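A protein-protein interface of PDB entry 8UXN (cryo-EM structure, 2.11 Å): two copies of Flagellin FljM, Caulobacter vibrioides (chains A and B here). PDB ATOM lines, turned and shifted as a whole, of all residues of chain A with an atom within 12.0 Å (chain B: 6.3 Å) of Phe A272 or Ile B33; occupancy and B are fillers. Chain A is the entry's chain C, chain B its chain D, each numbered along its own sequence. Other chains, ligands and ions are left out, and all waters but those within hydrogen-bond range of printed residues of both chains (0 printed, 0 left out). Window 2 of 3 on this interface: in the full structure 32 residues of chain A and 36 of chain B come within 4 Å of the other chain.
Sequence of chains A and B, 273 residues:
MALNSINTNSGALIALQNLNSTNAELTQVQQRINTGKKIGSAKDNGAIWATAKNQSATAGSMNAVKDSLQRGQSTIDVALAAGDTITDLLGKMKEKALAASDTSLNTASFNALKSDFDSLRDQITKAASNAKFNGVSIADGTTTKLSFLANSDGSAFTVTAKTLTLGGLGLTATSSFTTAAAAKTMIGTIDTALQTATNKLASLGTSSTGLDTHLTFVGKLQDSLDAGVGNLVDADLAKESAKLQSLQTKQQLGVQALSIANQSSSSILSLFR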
ATOM      1  N   LEU A   3      22.590  20.538 -30.109  1.00  0.00           N
ATOM      2  CA  LEU A   3      22.181  21.689 -29.312  1.00  0.00           C
ATOM      3  C   LEU A   3      23.105  21.882 -28.120  1.00  0.00           C
ATOM      4  O   LEU A   3      23.319  20.960 -27.343  1.00  0.00           O
ATOM      5  CB  LEU A   3      20.736  21.531 -28.838  1.00  0.00           C
ATOM      6  CG  LEU A   3      19.630  21.748 -29.877  1.00  0.00           C
ATOM      7  CD1 LEU A   3      18.294  21.971 -29.204  1.00  0.00           C
ATOM      8  CD2 LEU A   3      19.961  22.902 -30.811  1.00  0.00           C
ATOM      9  N   ASN A   4      23.645  23.092 -27.990  1.00  0.00           N
ATOM     10  CA  ASN A   4      24.587  23.433 -26.925  1.00  0.00           C
ATOM     11  C   ASN A   4      25.809  22.512 -26.937  1.00  0.00           C
ATOM     12  O   ASN A   4      26.370  22.183 -25.894  1.00  0.00           O
ATOM     13  CB  ASN A   4      23.898  23.418 -25.559  1.00  0.00           C
ATOM     14  CG  ASN A   4      22.599  24.201 -25.554  1.00  0.00           C
ATOM     15  OD1 ASN A   4      22.608  25.425 -25.578  1.00  0.00           O
ATOM     16  ND2 ASN A   4      21.481  23.497 -25.520  1.00  0.00           N
ATOM     17  N   SER A   5      26.205  22.079 -28.126  1.00  0.00           N
ATOM     18  CA  SER A   5      27.388  21.259 -28.319  1.00  0.00           C
ATOM     19  C   SER A   5      28.657  22.102 -28.318  1.00  0.00           C
ATOM     20  O   SER A   5      28.657  23.259 -28.734  1.00  0.00           O
ATOM     21  CB  SER A   5      27.272  20.488 -29.632  1.00  0.00           C
ATOM     22  OG  SER A   5      28.514  19.976 -30.054  1.00  0.00           O
ATOM     23  N   ILE A   6      29.751  21.506 -27.855  1.00  0.00           N
ATOM     24  CA  ILE A   6      31.074  22.102 -28.006  1.00  0.00           C
ATOM     25  C   ILE A   6      31.916  21.412 -29.059  1.00  0.00           C
ATOM     26  O   ILE A   6      33.019  21.888 -29.349  1.00  0.00           O
ATOM     27  CB  ILE A   6      31.847  22.132 -26.672  1.00  0.00           C
ATOM     28  CG1 ILE A   6      31.953  20.724 -26.081  1.00  0.00           C
ATOM     29  CG2 ILE A   6      31.227  23.124 -25.729  1.00  0.00           C
ATOM     30  CD1 ILE A   6      32.666  20.663 -24.770  1.00  0.00           C
ATOM     31  N   ASN A   7      31.458  20.302 -29.622  1.00  0.00           N
ATOM     32  CA  ASN A   7      32.247  19.586 -30.613  1.00  0.00           C
ATOM     33  C   ASN A   7      31.840  19.883 -32.043  1.00  0.00           C
ATOM     34  O   ASN A   7      32.684  19.844 -32.935  1.00  0.00           O
ATOM     35  CB  ASN A   7      32.150  18.078 -30.374  1.00  0.00           C
ATOM     36  CG  ASN A   7      32.855  17.649 -29.119  1.00  0.00           C
ATOM     37  OD1 ASN A   7      33.899  18.179 -28.781  1.00  0.00           O
ATOM     38  ND2 ASN A   7      32.289  16.691 -28.423  1.00  0.00           N
ATOM     39  N   THR A   8      30.574  20.175 -32.287  1.00  0.00           N
ATOM     40  CA  THR A   8      30.071  20.389 -33.633  1.00  0.00           C
ATOM     41  C   THR A   8      29.363  21.726 -33.671  1.00  0.00           C
ATOM     42  O   THR A   8      28.467  21.981 -32.864  1.00  0.00           O
ATOM     43  CB  THR A   8      29.106  19.275 -34.057  1.00  0.00           C
ATOM     44  OG1 THR A   8      29.707  17.998 -33.826  1.00  0.00           O
ATOM     45  CG2 THR A   8      28.764  19.405 -35.528  1.00  0.00           C
ATOM     46  N   SER A 264      29.157  30.559 -30.598  1.00  0.00           N
ATOM     47  CA  SER A 264      28.107  29.806 -29.920  1.00  0.00           C
ATOM     48  C   SER A 264      28.648  28.964 -28.771  1.00  0.00           C
ATOM     49  O   SER A 264      27.984  28.814 -27.744  1.00  0.00           O
ATOM     50  CB  SER A 264      27.377  28.921 -30.922  1.00  0.00           C
ATOM     51  OG  SER A 264      28.228  27.903 -31.399  1.00  0.00           O
ATOM     52  N   SER A 265      29.847  28.404 -28.920  1.00  0.00           N
ATOM     53  CA  SER A 265      30.357  27.510 -27.886  1.00  0.00           C
ATOM     54  C   SER A 265      30.638  28.248 -26.589  1.00  0.00           C
ATOM     55  O   SER A 265      30.502  27.669 -25.509  1.00  0.00           O
ATOM     56  CB  SER A 265      31.620  26.795 -28.365  1.00  0.00           C
ATOM     57  OG  SER A 265      32.690  27.705 -28.536  1.00  0.00           O
ATOM     58  N   SER A 266      31.010  29.521 -26.667  1.00  0.00           N
ATOM     59  CA  SER A 266      31.407  30.250 -25.478  1.00  0.00           C
ATOM     60  C   SER A 266      30.226  30.683 -24.622  1.00  0.00           C
ATOM     61  O   SER A 266      30.436  31.119 -23.489  1.00  0.00           O
ATOM     62  CB  SER A 266      32.238  31.474 -25.865  1.00  0.00           C
ATOM     63  OG  SER A 266      31.426  32.503 -26.391  1.00  0.00           O
ATOM     64  N   SER A 267      28.999  30.597 -25.139  1.00  0.00           N
ATOM     65  CA  SER A 267      27.843  31.005 -24.351  1.00  0.00           C
ATOM     66  C   SER A 267      27.632  30.121 -23.131  1.00  0.00           C
ATOM     67  O   SER A 267      27.218  30.619 -22.083  1.00  0.00           O
ATOM     68  CB  SER A 267      26.588  31.006 -25.220  1.00  0.00           C
ATOM     69  OG  SER A 267      26.782  31.779 -26.385  1.00  0.00           O
ATOM     70  N   ILE A 268      27.922  28.820 -23.230  1.00  0.00           N
ATOM     71  CA  ILE A 268      27.657  27.911 -22.119  1.00  0.00           C
ATOM     72  C   ILE A 268      28.799  27.843 -21.122  1.00  0.00           C
ATOM     73  O   ILE A 268      28.669  27.166 -20.097  1.00  0.00           O
ATOM     74  CB  ILE A 268      27.294  26.493 -22.614  1.00  0.00           C
ATOM     75  CG1 ILE A 268      28.362  25.915 -23.553  1.00  0.00           C
ATOM     76  CG2 ILE A 268      25.908  26.486 -23.230  1.00  0.00           C
ATOM     77  CD1 ILE A 268      29.562  25.305 -22.871  1.00  0.00           C
ATOM     78  N   LEU A 269      29.914  28.512 -21.391  1.00  0.00           N
ATOM     79  CA  LEU A 269      31.010  28.526 -20.433  1.00  0.00           C
ATOM     80  C   LEU A 269      30.579  29.145 -19.114  1.00  0.00           C
ATOM     81  O   LEU A 269      31.089  28.774 -18.055  1.00  0.00           O
ATOM     82  CB  LEU A 269      32.183  29.292 -21.029  1.00  0.00           C
ATOM     83  CG  LEU A 269      33.613  28.810 -20.824  1.00  0.00           C
ATOM     84  CD1 LEU A 269      33.710  27.308 -20.918  1.00  0.00           C
ATOM     85  CD2 LEU A 269      34.476  29.466 -21.867  1.00  0.00           C
ATOM     86  N   SER A 270      29.619  30.064 -19.160  1.00  0.00           N
ATOM     87  CA  SER A 270      29.111  30.711 -17.962  1.00  0.00           C
ATOM     88  C   SER A 270      28.360  29.755 -17.046  1.00  0.00           C
ATOM     89  O   SER A 270      28.270  30.016 -15.845  1.00  0.00           O
ATOM     90  CB  SER A 270      28.208  31.872 -18.361  1.00  0.00           C
ATOM     91  OG  SER A 270      27.610  32.449 -17.225  1.00  0.00           O
ATOM     92  N   LEU A 271      27.827  28.657 -17.574  1.00  0.00           N
ATOM     93  CA  LEU A 271      27.074  27.723 -16.754  1.00  0.00           C
ATOM     94  C   LEU A 271      27.959  26.855 -15.880  1.00  0.00           C
ATOM     95  O   LEU A 271      27.442  26.160 -15.004  1.00  0.00           O
ATOM     96  CB  LEU A 271      26.206  26.835 -17.633  1.00  0.00           C
ATOM     97  CG  LEU A 271      25.170  27.559 -18.478  1.00  0.00           C
ATOM     98  CD1 LEU A 271      24.550  26.595 -19.446  1.00  0.00           C
ATOM     99  CD2 LEU A 271      24.118  28.202 -17.590  1.00  0.00           C
ATOM    100  N   PHE A 272      29.263  26.864 -16.098  1.00  0.00           N
ATOM    101  CA  PHE A 272      30.165  26.048 -15.314  1.00  0.00           C
ATOM    102  C   PHE A 272      31.138  26.933 -14.550  1.00  0.00           C
ATOM    103  O   PHE A 272      31.462  26.658 -13.402  1.00  0.00           O
ATOM    104  CB  PHE A 272      30.918  25.070 -16.214  1.00  0.00           C
ATOM    105  CG  PHE A 272      30.029  24.107 -16.932  1.00  0.00           C
ATOM    106  CD1 PHE A 272      29.643  22.930 -16.333  1.00  0.00           C
ATOM    107  CD2 PHE A 272      29.570  24.383 -18.198  1.00  0.00           C
ATOM    108  CE1 PHE A 272      28.828  22.053 -16.983  1.00  0.00           C
ATOM    109  CE2 PHE A 272      28.757  23.504 -18.849  1.00  0.00           C
ATOM    110  CZ  PHE A 272      28.387  22.338 -18.241  1.00  0.00           C
ATOM    111  N   GLN B  28      29.905  10.038 -14.474  1.00  0.00           N
ATOM    112  CA  GLN B  28      29.381  10.078 -15.835  1.00  0.00           C
ATOM    113  C   GLN B  28      29.222  11.515 -16.332  1.00  0.00           C
ATOM    114  O   GLN B  28      29.599  11.837 -17.469  1.00  0.00           O
ATOM    115  CB  GLN B  28      28.057   9.330 -15.887  1.00  0.00           C
ATOM    116  CG  GLN B  28      27.351   9.356 -17.225  1.00  0.00           C
ATOM    117  CD  GLN B  28      26.098   8.504 -17.221  1.00  0.00           C
ATOM    118  OE1 GLN B  28      25.822   7.801 -16.253  1.00  0.00           O
ATOM    119  NE2 GLN B  28      25.333   8.566 -18.300  1.00  0.00           N
ATOM    120  N   VAL B  29      28.692  12.399 -15.485  1.00  0.00           N
ATOM    121  CA  VAL B  29      28.503  13.781 -15.913  1.00  0.00           C
ATOM    122  C   VAL B  29      29.846  14.465 -16.143  1.00  0.00           C
ATOM    123  O   VAL B  29      29.999  15.255 -17.081  1.00  0.00           O
ATOM    124  CB  VAL B  29      27.627  14.546 -14.904  1.00  0.00           C
ATOM    125  CG1 VAL B  29      27.545  15.999 -15.257  1.00  0.00           C
ATOM    126  CG2 VAL B  29      26.245  13.972 -14.892  1.00  0.00           C
ATOM    127  N   GLN B  30      30.853  14.145 -15.327  1.00  0.00           N
ATOM    128  CA  GLN B  30      32.179  14.711 -15.557  1.00  0.00           C
ATOM    129  C   GLN B  30      32.755  14.266 -16.894  1.00  0.00           C
ATOM    130  O   GLN B  30      33.396  15.057 -17.596  1.00  0.00           O
ATOM    131  CB  GLN B  30      33.132  14.318 -14.433  1.00  0.00           C
ATOM    132  CG  GLN B  30      32.929  15.044 -13.130  1.00  0.00           C
ATOM    133  CD  GLN B  30      33.677  14.380 -11.993  1.00  0.00           C
ATOM    134  OE1 GLN B  30      33.207  14.350 -10.858  1.00  0.00           O
ATOM    135  NE2 GLN B  30      34.843  13.831 -12.296  1.00  0.00           N
ATOM    136  N   GLN B  31      32.546  13.004 -17.263  1.00  0.00           N
ATOM    137  CA  GLN B  31      33.049  12.558 -18.558  1.00  0.00           C
ATOM    138  C   GLN B  31      32.346  13.283 -19.697  1.00  0.00           C
ATOM    139  O   GLN B  31      32.995  13.703 -20.663  1.00  0.00           O
ATOM    140  CB  GLN B  31      32.888  11.050 -18.697  1.00  0.00           C
ATOM    141  CG  GLN B  31      33.768  10.261 -17.762  1.00  0.00           C
ATOM    142  CD  GLN B  31      33.408   8.796 -17.721  1.00  0.00           C
ATOM    143  OE1 GLN B  31      32.407   8.374 -18.298  1.00  0.00           O
ATOM    144  NE2 GLN B  31      34.213   8.012 -17.019  1.00  0.00           N
ATOM    145  N   ARG B  32      31.034  13.490 -19.574  1.00  0.00           N
ATOM    146  CA  ARG B  32      30.326  14.229 -20.615  1.00  0.00           C
ATOM    147  C   ARG B  32      30.830  15.660 -20.720  1.00  0.00           C
ATOM    148  O   ARG B  32      30.908  16.217 -21.817  1.00  0.00           O
ATOM    149  CB  ARG B  32      28.827  14.229 -20.353  1.00  0.00           C
ATOM    150  CG  ARG B  32      28.171  12.901 -20.520  1.00  0.00           C
ATOM    151  CD  ARG B  32      26.680  13.042 -20.523  1.00  0.00           C
ATOM    152  NE  ARG B  32      26.031  11.742 -20.544  1.00  0.00           N
ATOM    153  CZ  ARG B  32      24.738  11.547 -20.749  1.00  0.00           C
ATOM    154  NH1 ARG B  32      23.911  12.556 -20.958  1.00  0.00           N
ATOM    155  NH2 ARG B  32      24.263  10.309 -20.745  1.00  0.00           N
ATOM    156  N   ILE B  33      31.198  16.263 -19.595  1.00  0.00           N
ATOM    157  CA  ILE B  33      31.646  17.647 -19.633  1.00  0.00           C
ATOM    158  C   ILE B  33      33.031  17.752 -20.257  1.00  0.00           C
ATOM    159  O   ILE B  33      33.282  18.641 -21.077  1.00  0.00           O
ATOM    160  CB  ILE B  33      31.609  18.266 -18.224  1.00  0.00           C
ATOM    161  CG1 ILE B  33      30.172  18.543 -17.802  1.00  0.00           C
ATOM    162  CG2 ILE B  33      32.402  19.541 -18.183  1.00  0.00           C
ATOM    163  CD1 ILE B  33      30.015  18.712 -16.333  1.00  0.00           C
ATOM    164  N   ASN B  34      33.956  16.868 -19.885  1.00  0.00           N
ATOM    165  CA  ASN B  34      35.295  17.050 -20.433  1.00  0.00           C
ATOM    166  C   ASN B  34      35.419  16.552 -21.871  1.00  0.00           C
ATOM    167  O   ASN B  34      36.261  17.060 -22.611  1.00  0.00           O
ATOM    168  CB  ASN B  34      36.368  16.417 -19.538  1.00  0.00           C
ATOM    169  CG  ASN B  34      36.134  14.966 -19.251  1.00  0.00           C
ATOM    170  OD1 ASN B  34      35.771  14.199 -20.127  1.00  0.00           O
ATOM    171  ND2 ASN B  34      36.379  14.566 -18.009  1.00  0.00           N
ATOM    172  N   THR B  35      34.591  15.605 -22.308  1.00  0.00           N
ATOM    173  CA  THR B  35      34.660  15.204 -23.709  1.00  0.00           C
ATOM    174  C   THR B  35      33.692  15.963 -24.600  1.00  0.00           C
ATOM    175  O   THR B  35      33.905  16.030 -25.811  1.00  0.00           O
ATOM    176  CB  THR B  35      34.383  13.709 -23.865  1.00  0.00           C
ATOM    177  OG1 THR B  35      33.075  13.412 -23.370  1.00  0.00           O
ATOM    178  CG2 THR B  35      35.412  12.887 -23.120  1.00  0.00           C
ATOM    179  N   GLY B  36      32.622  16.512 -24.043  1.00  0.00           N
ATOM    180  CA  GLY B  36      31.579  17.054 -24.880  1.00  0.00           C
ATOM    181  C   GLY B  36      30.711  16.010 -25.535  1.00  0.00           C
ATOM    182  O   GLY B  36      29.991  16.325 -26.474  1.00  0.00           O
ATOM    183  N   LYS B  37      30.765  14.767 -25.074  1.00  0.00           N
ATOM    184  CA  LYS B  37      30.079  13.661 -25.725  1.00  0.00           C
ATOM    185  C   LYS B  37      29.210  12.921 -24.727  1.00  0.00           C
ATOM    186  O   LYS B  37      29.682  12.543 -23.655  1.00  0.00           O
ATOM    187  CB  LYS B  37      31.076  12.688 -26.347  1.00  0.00           C
ATOM    188  CG  LYS B  37      31.836  13.251 -27.510  1.00  0.00           C
ATOM    189  CD  LYS B  37      32.801  12.242 -28.041  1.00  0.00           C
ATOM    190  CE  LYS B  37      33.692  12.849 -29.082  1.00  0.00           C
ATOM    191  NZ  LYS B  37      32.886  13.434 -30.159  1.00  0.00           N
ATOM    192  N   ALA B 235      27.206  15.767 -26.355  1.00  0.00           N
ATOM    193  CA  ALA B 235      26.456  16.116 -25.161  1.00  0.00           C
ATOM    194  C   ALA B 235      25.817  17.492 -25.299  1.00  0.00           C
ATOM    195  O   ALA B 235      26.343  18.384 -25.963  1.00  0.00           O
ATOM    196  CB  ALA B 235      27.367  16.085 -23.933  1.00  0.00           C
ATOM    197  N   LEU B 237      25.513  20.434 -23.263  1.00  0.00           N
ATOM    198  CA  LEU B 237      26.204  20.866 -22.054  1.00  0.00           C
ATOM    199  C   LEU B 237      25.347  21.744 -21.161  1.00  0.00           C
ATOM    200  O   LEU B 237      25.563  21.771 -19.945  1.00  0.00           O
ATOM    201  CB  LEU B 237      27.491  21.571 -22.423  1.00  0.00           C
ATOM    202  CG  LEU B 237      28.453  20.495 -22.891  1.00  0.00           C
ATOM    203  CD1 LEU B 237      29.413  21.131 -23.772  1.00  0.00           C
ATOM    204  CD2 LEU B 237      29.155  19.847 -21.737  1.00  0.00           C
ATOM    205  N   ALA B 238      24.379  22.462 -21.727  1.00  0.00           N
ATOM    206  CA  ALA B 238      23.483  23.244 -20.889  1.00  0.00           C
ATOM    207  C   ALA B 238      22.676  22.343 -19.967  1.00  0.00           C
ATOM    208  O   ALA B 238      22.482  22.666 -18.795  1.00  0.00           O
ATOM    209  CB  ALA B 238      22.571  24.110 -21.755  1.00  0.00           C
ATOM    210  N   GLU B 240      23.742  19.343 -18.993  1.00  0.00           N
ATOM    211  CA  GLU B 240      24.717  18.759 -18.081  1.00  0.00           C
ATOM    212  C   GLU B 240      25.051  19.691 -16.927  1.00  0.00           C
ATOM    213  O   GLU B 240      25.368  19.215 -15.840  1.00  0.00           O
ATOM    214  CB  GLU B 240      25.997  18.381 -18.824  1.00  0.00           C
ATOM    215  CG  GLU B 240      25.840  17.341 -19.909  1.00  0.00           C
ATOM    216  CD  GLU B 240      25.047  16.128 -19.474  1.00  0.00           C
ATOM    217  OE1 GLU B 240      25.254  15.641 -18.348  1.00  0.00           O
ATOM    218  OE2 GLU B 240      24.213  15.649 -20.263  1.00  0.00           O
ATOM    219  N   SER B 241      25.012  21.008 -17.135  1.00  0.00           N
ATOM    220  CA  SER B 241      25.321  21.914 -16.031  1.00  0.00           C
ATOM    221  C   SER B 241      24.293  21.789 -14.906  1.00  0.00           C
ATOM    222  O   SER B 241      24.653  21.769 -13.718  1.00  0.00           O
ATOM    223  CB  SER B 241      25.412  23.351 -16.540  1.00  0.00           C
ATOM    224  OG  SER B 241      24.176  23.803 -17.048  1.00  0.00           O
ATOM    225  N   ALA B 242      23.020  21.633 -15.262  1.00  0.00           N
ATOM    226  CA  ALA B 242      21.995  21.413 -14.252  1.00  0.00           C
ATOM    227  C   ALA B 242      22.183  20.074 -13.560  1.00  0.00           C
ATOM    228  O   ALA B 242      22.081  19.981 -12.324  1.00  0.00           O
ATOM    229  CB  ALA B 242      20.611  21.489 -14.885  1.00  0.00           C
ATOM    230  N   LEU B 244      24.923  18.527 -13.121  1.00  0.00           N
ATOM    231  CA  LEU B 244      26.114  18.596 -12.290  1.00  0.00           C
ATOM    232  C   LEU B 244      25.812  19.267 -10.960  1.00  0.00           C
ATOM    233  O   LEU B 244      26.201  18.764  -9.899  1.00  0.00           O
ATOM    234  CB  LEU B 244      27.222  19.342 -13.029  1.00  0.00           C
ATOM    235  CG  LEU B 244      28.445  19.744 -12.210  1.00  0.00           C
ATOM    236  CD1 LEU B 244      29.216  18.523 -11.754  1.00  0.00           C
ATOM    237  CD2 LEU B 244      29.338  20.678 -12.993  1.00  0.00           C
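O of Asn A4 sits at hydrogen-bond distance from N of Leu B237. ND2 of Asn A7 lies within hydrogen-bond range of O of Thr B35, 3.1 Å away. The side-chain amide nitrogen (ND2) of Asn A7 lies within hydrogen-bond range of the backbone carbonyl oxygen (O) of Gly B36.
The backbone NH (N) of Asn A7 is in hydrogen-bond range of the side-chain hydroxyl (OG) of Ser A5 (3.0 Å). The side-chain hydroxyl (OG) of Ser A5 sits at hydrogen-bond distance from the backbone NH (N) of Thr A8 (3.0 Å). The side-chain hydroxyl (OG1) of Thr B35 lies within hydrogen-bond range of the backbone carbonyl oxygen (O) of Gln B31 (2.7 Å). OG1 of Thr B35 is in hydrogen-bond range of N of Lys B37 (3.2 Å). The backbone carbonyl oxygen (O) of Gly B36 lies within hydrogen-bond range of the backbone NH (N) of Ala B235, at 2.8 Å. O of Ala B238 is in hydrogen-bond range of OG of Ser B241.
Among the printed residues, merely in contact across the chains: Asn A4 with Ala B235 (3.8 Å), Asn A4 with Ala B238 (3.8 Å), Ser A5 with Ala B235 (3.9 Å), Ile A6 with Gly B36 (3.8 Å), Ile A6 with Leu B237 (3.3 Å), Asn A7 with Lys B37 (3.6 Å), Leu A271 with Ala B238 (3.8 Å), Leu A271 with Ser B241 (3.7 Å), Phe A272 with Ile B33 (3.6 Å), Phe A272 with Leu B237 (3.3 Å) and Phe A272 with Ser B241 (3.6 Å).
Of chain B, only Ile B33, Leu B237 and Ser B241 come within 4 Å of Phe A272. Of chain A, only Phe A272 comes within 4 Å of Ile B33. No residue of chain A comes within 4 Å of Val B29. No residue of chain A comes within 4 Å of Asn B34. Of chain A, only Ile A6 and Asn A7 come within 4 Å of Gly B36. Of chain A, only Asn A4, Ile A6 and Phe A272 come within 4 Å of Leu B237. Of the printed residues of chain A, Ala B238 touches Asn A4 (3.8 Å) and Leu A271 (3.8 Å). No residue of chain A comes within 4 Å of Glu B240. Of chain A, only Leu A271 and Phe A272 come within 4 Å of Ser B241. Of the printed residues of chain A, Ala B235 touches Asn A4 and Ser A5. Printed residues of chain B within 4 Å of Asn A7: Thr B35 (3.1 Å), Gly B36 (3.0 Å) and Lys B37 (3.6 Å). Of the printed residues of chain A, Lys B37 touches Asn A7. Of the printed residues of chain B, Ile A6 touches Gly B36 and Leu B237. Printed residues of chain B within 4 Å of Leu A271: Ala B238 (3.8 Å) and Ser B241 (3.7 Å). The nearest printed residue of chain B that does not touch Ser A5 is Leu B237 (4.7 Å).
Hydrophobic or aromatic side chains of chain A within 4 Å of the printed part of chain B: Ile A6, Leu A271 and Phe A272. Among the printed residues, 14 pairs touch across the chains.
No position is printed for both chains.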
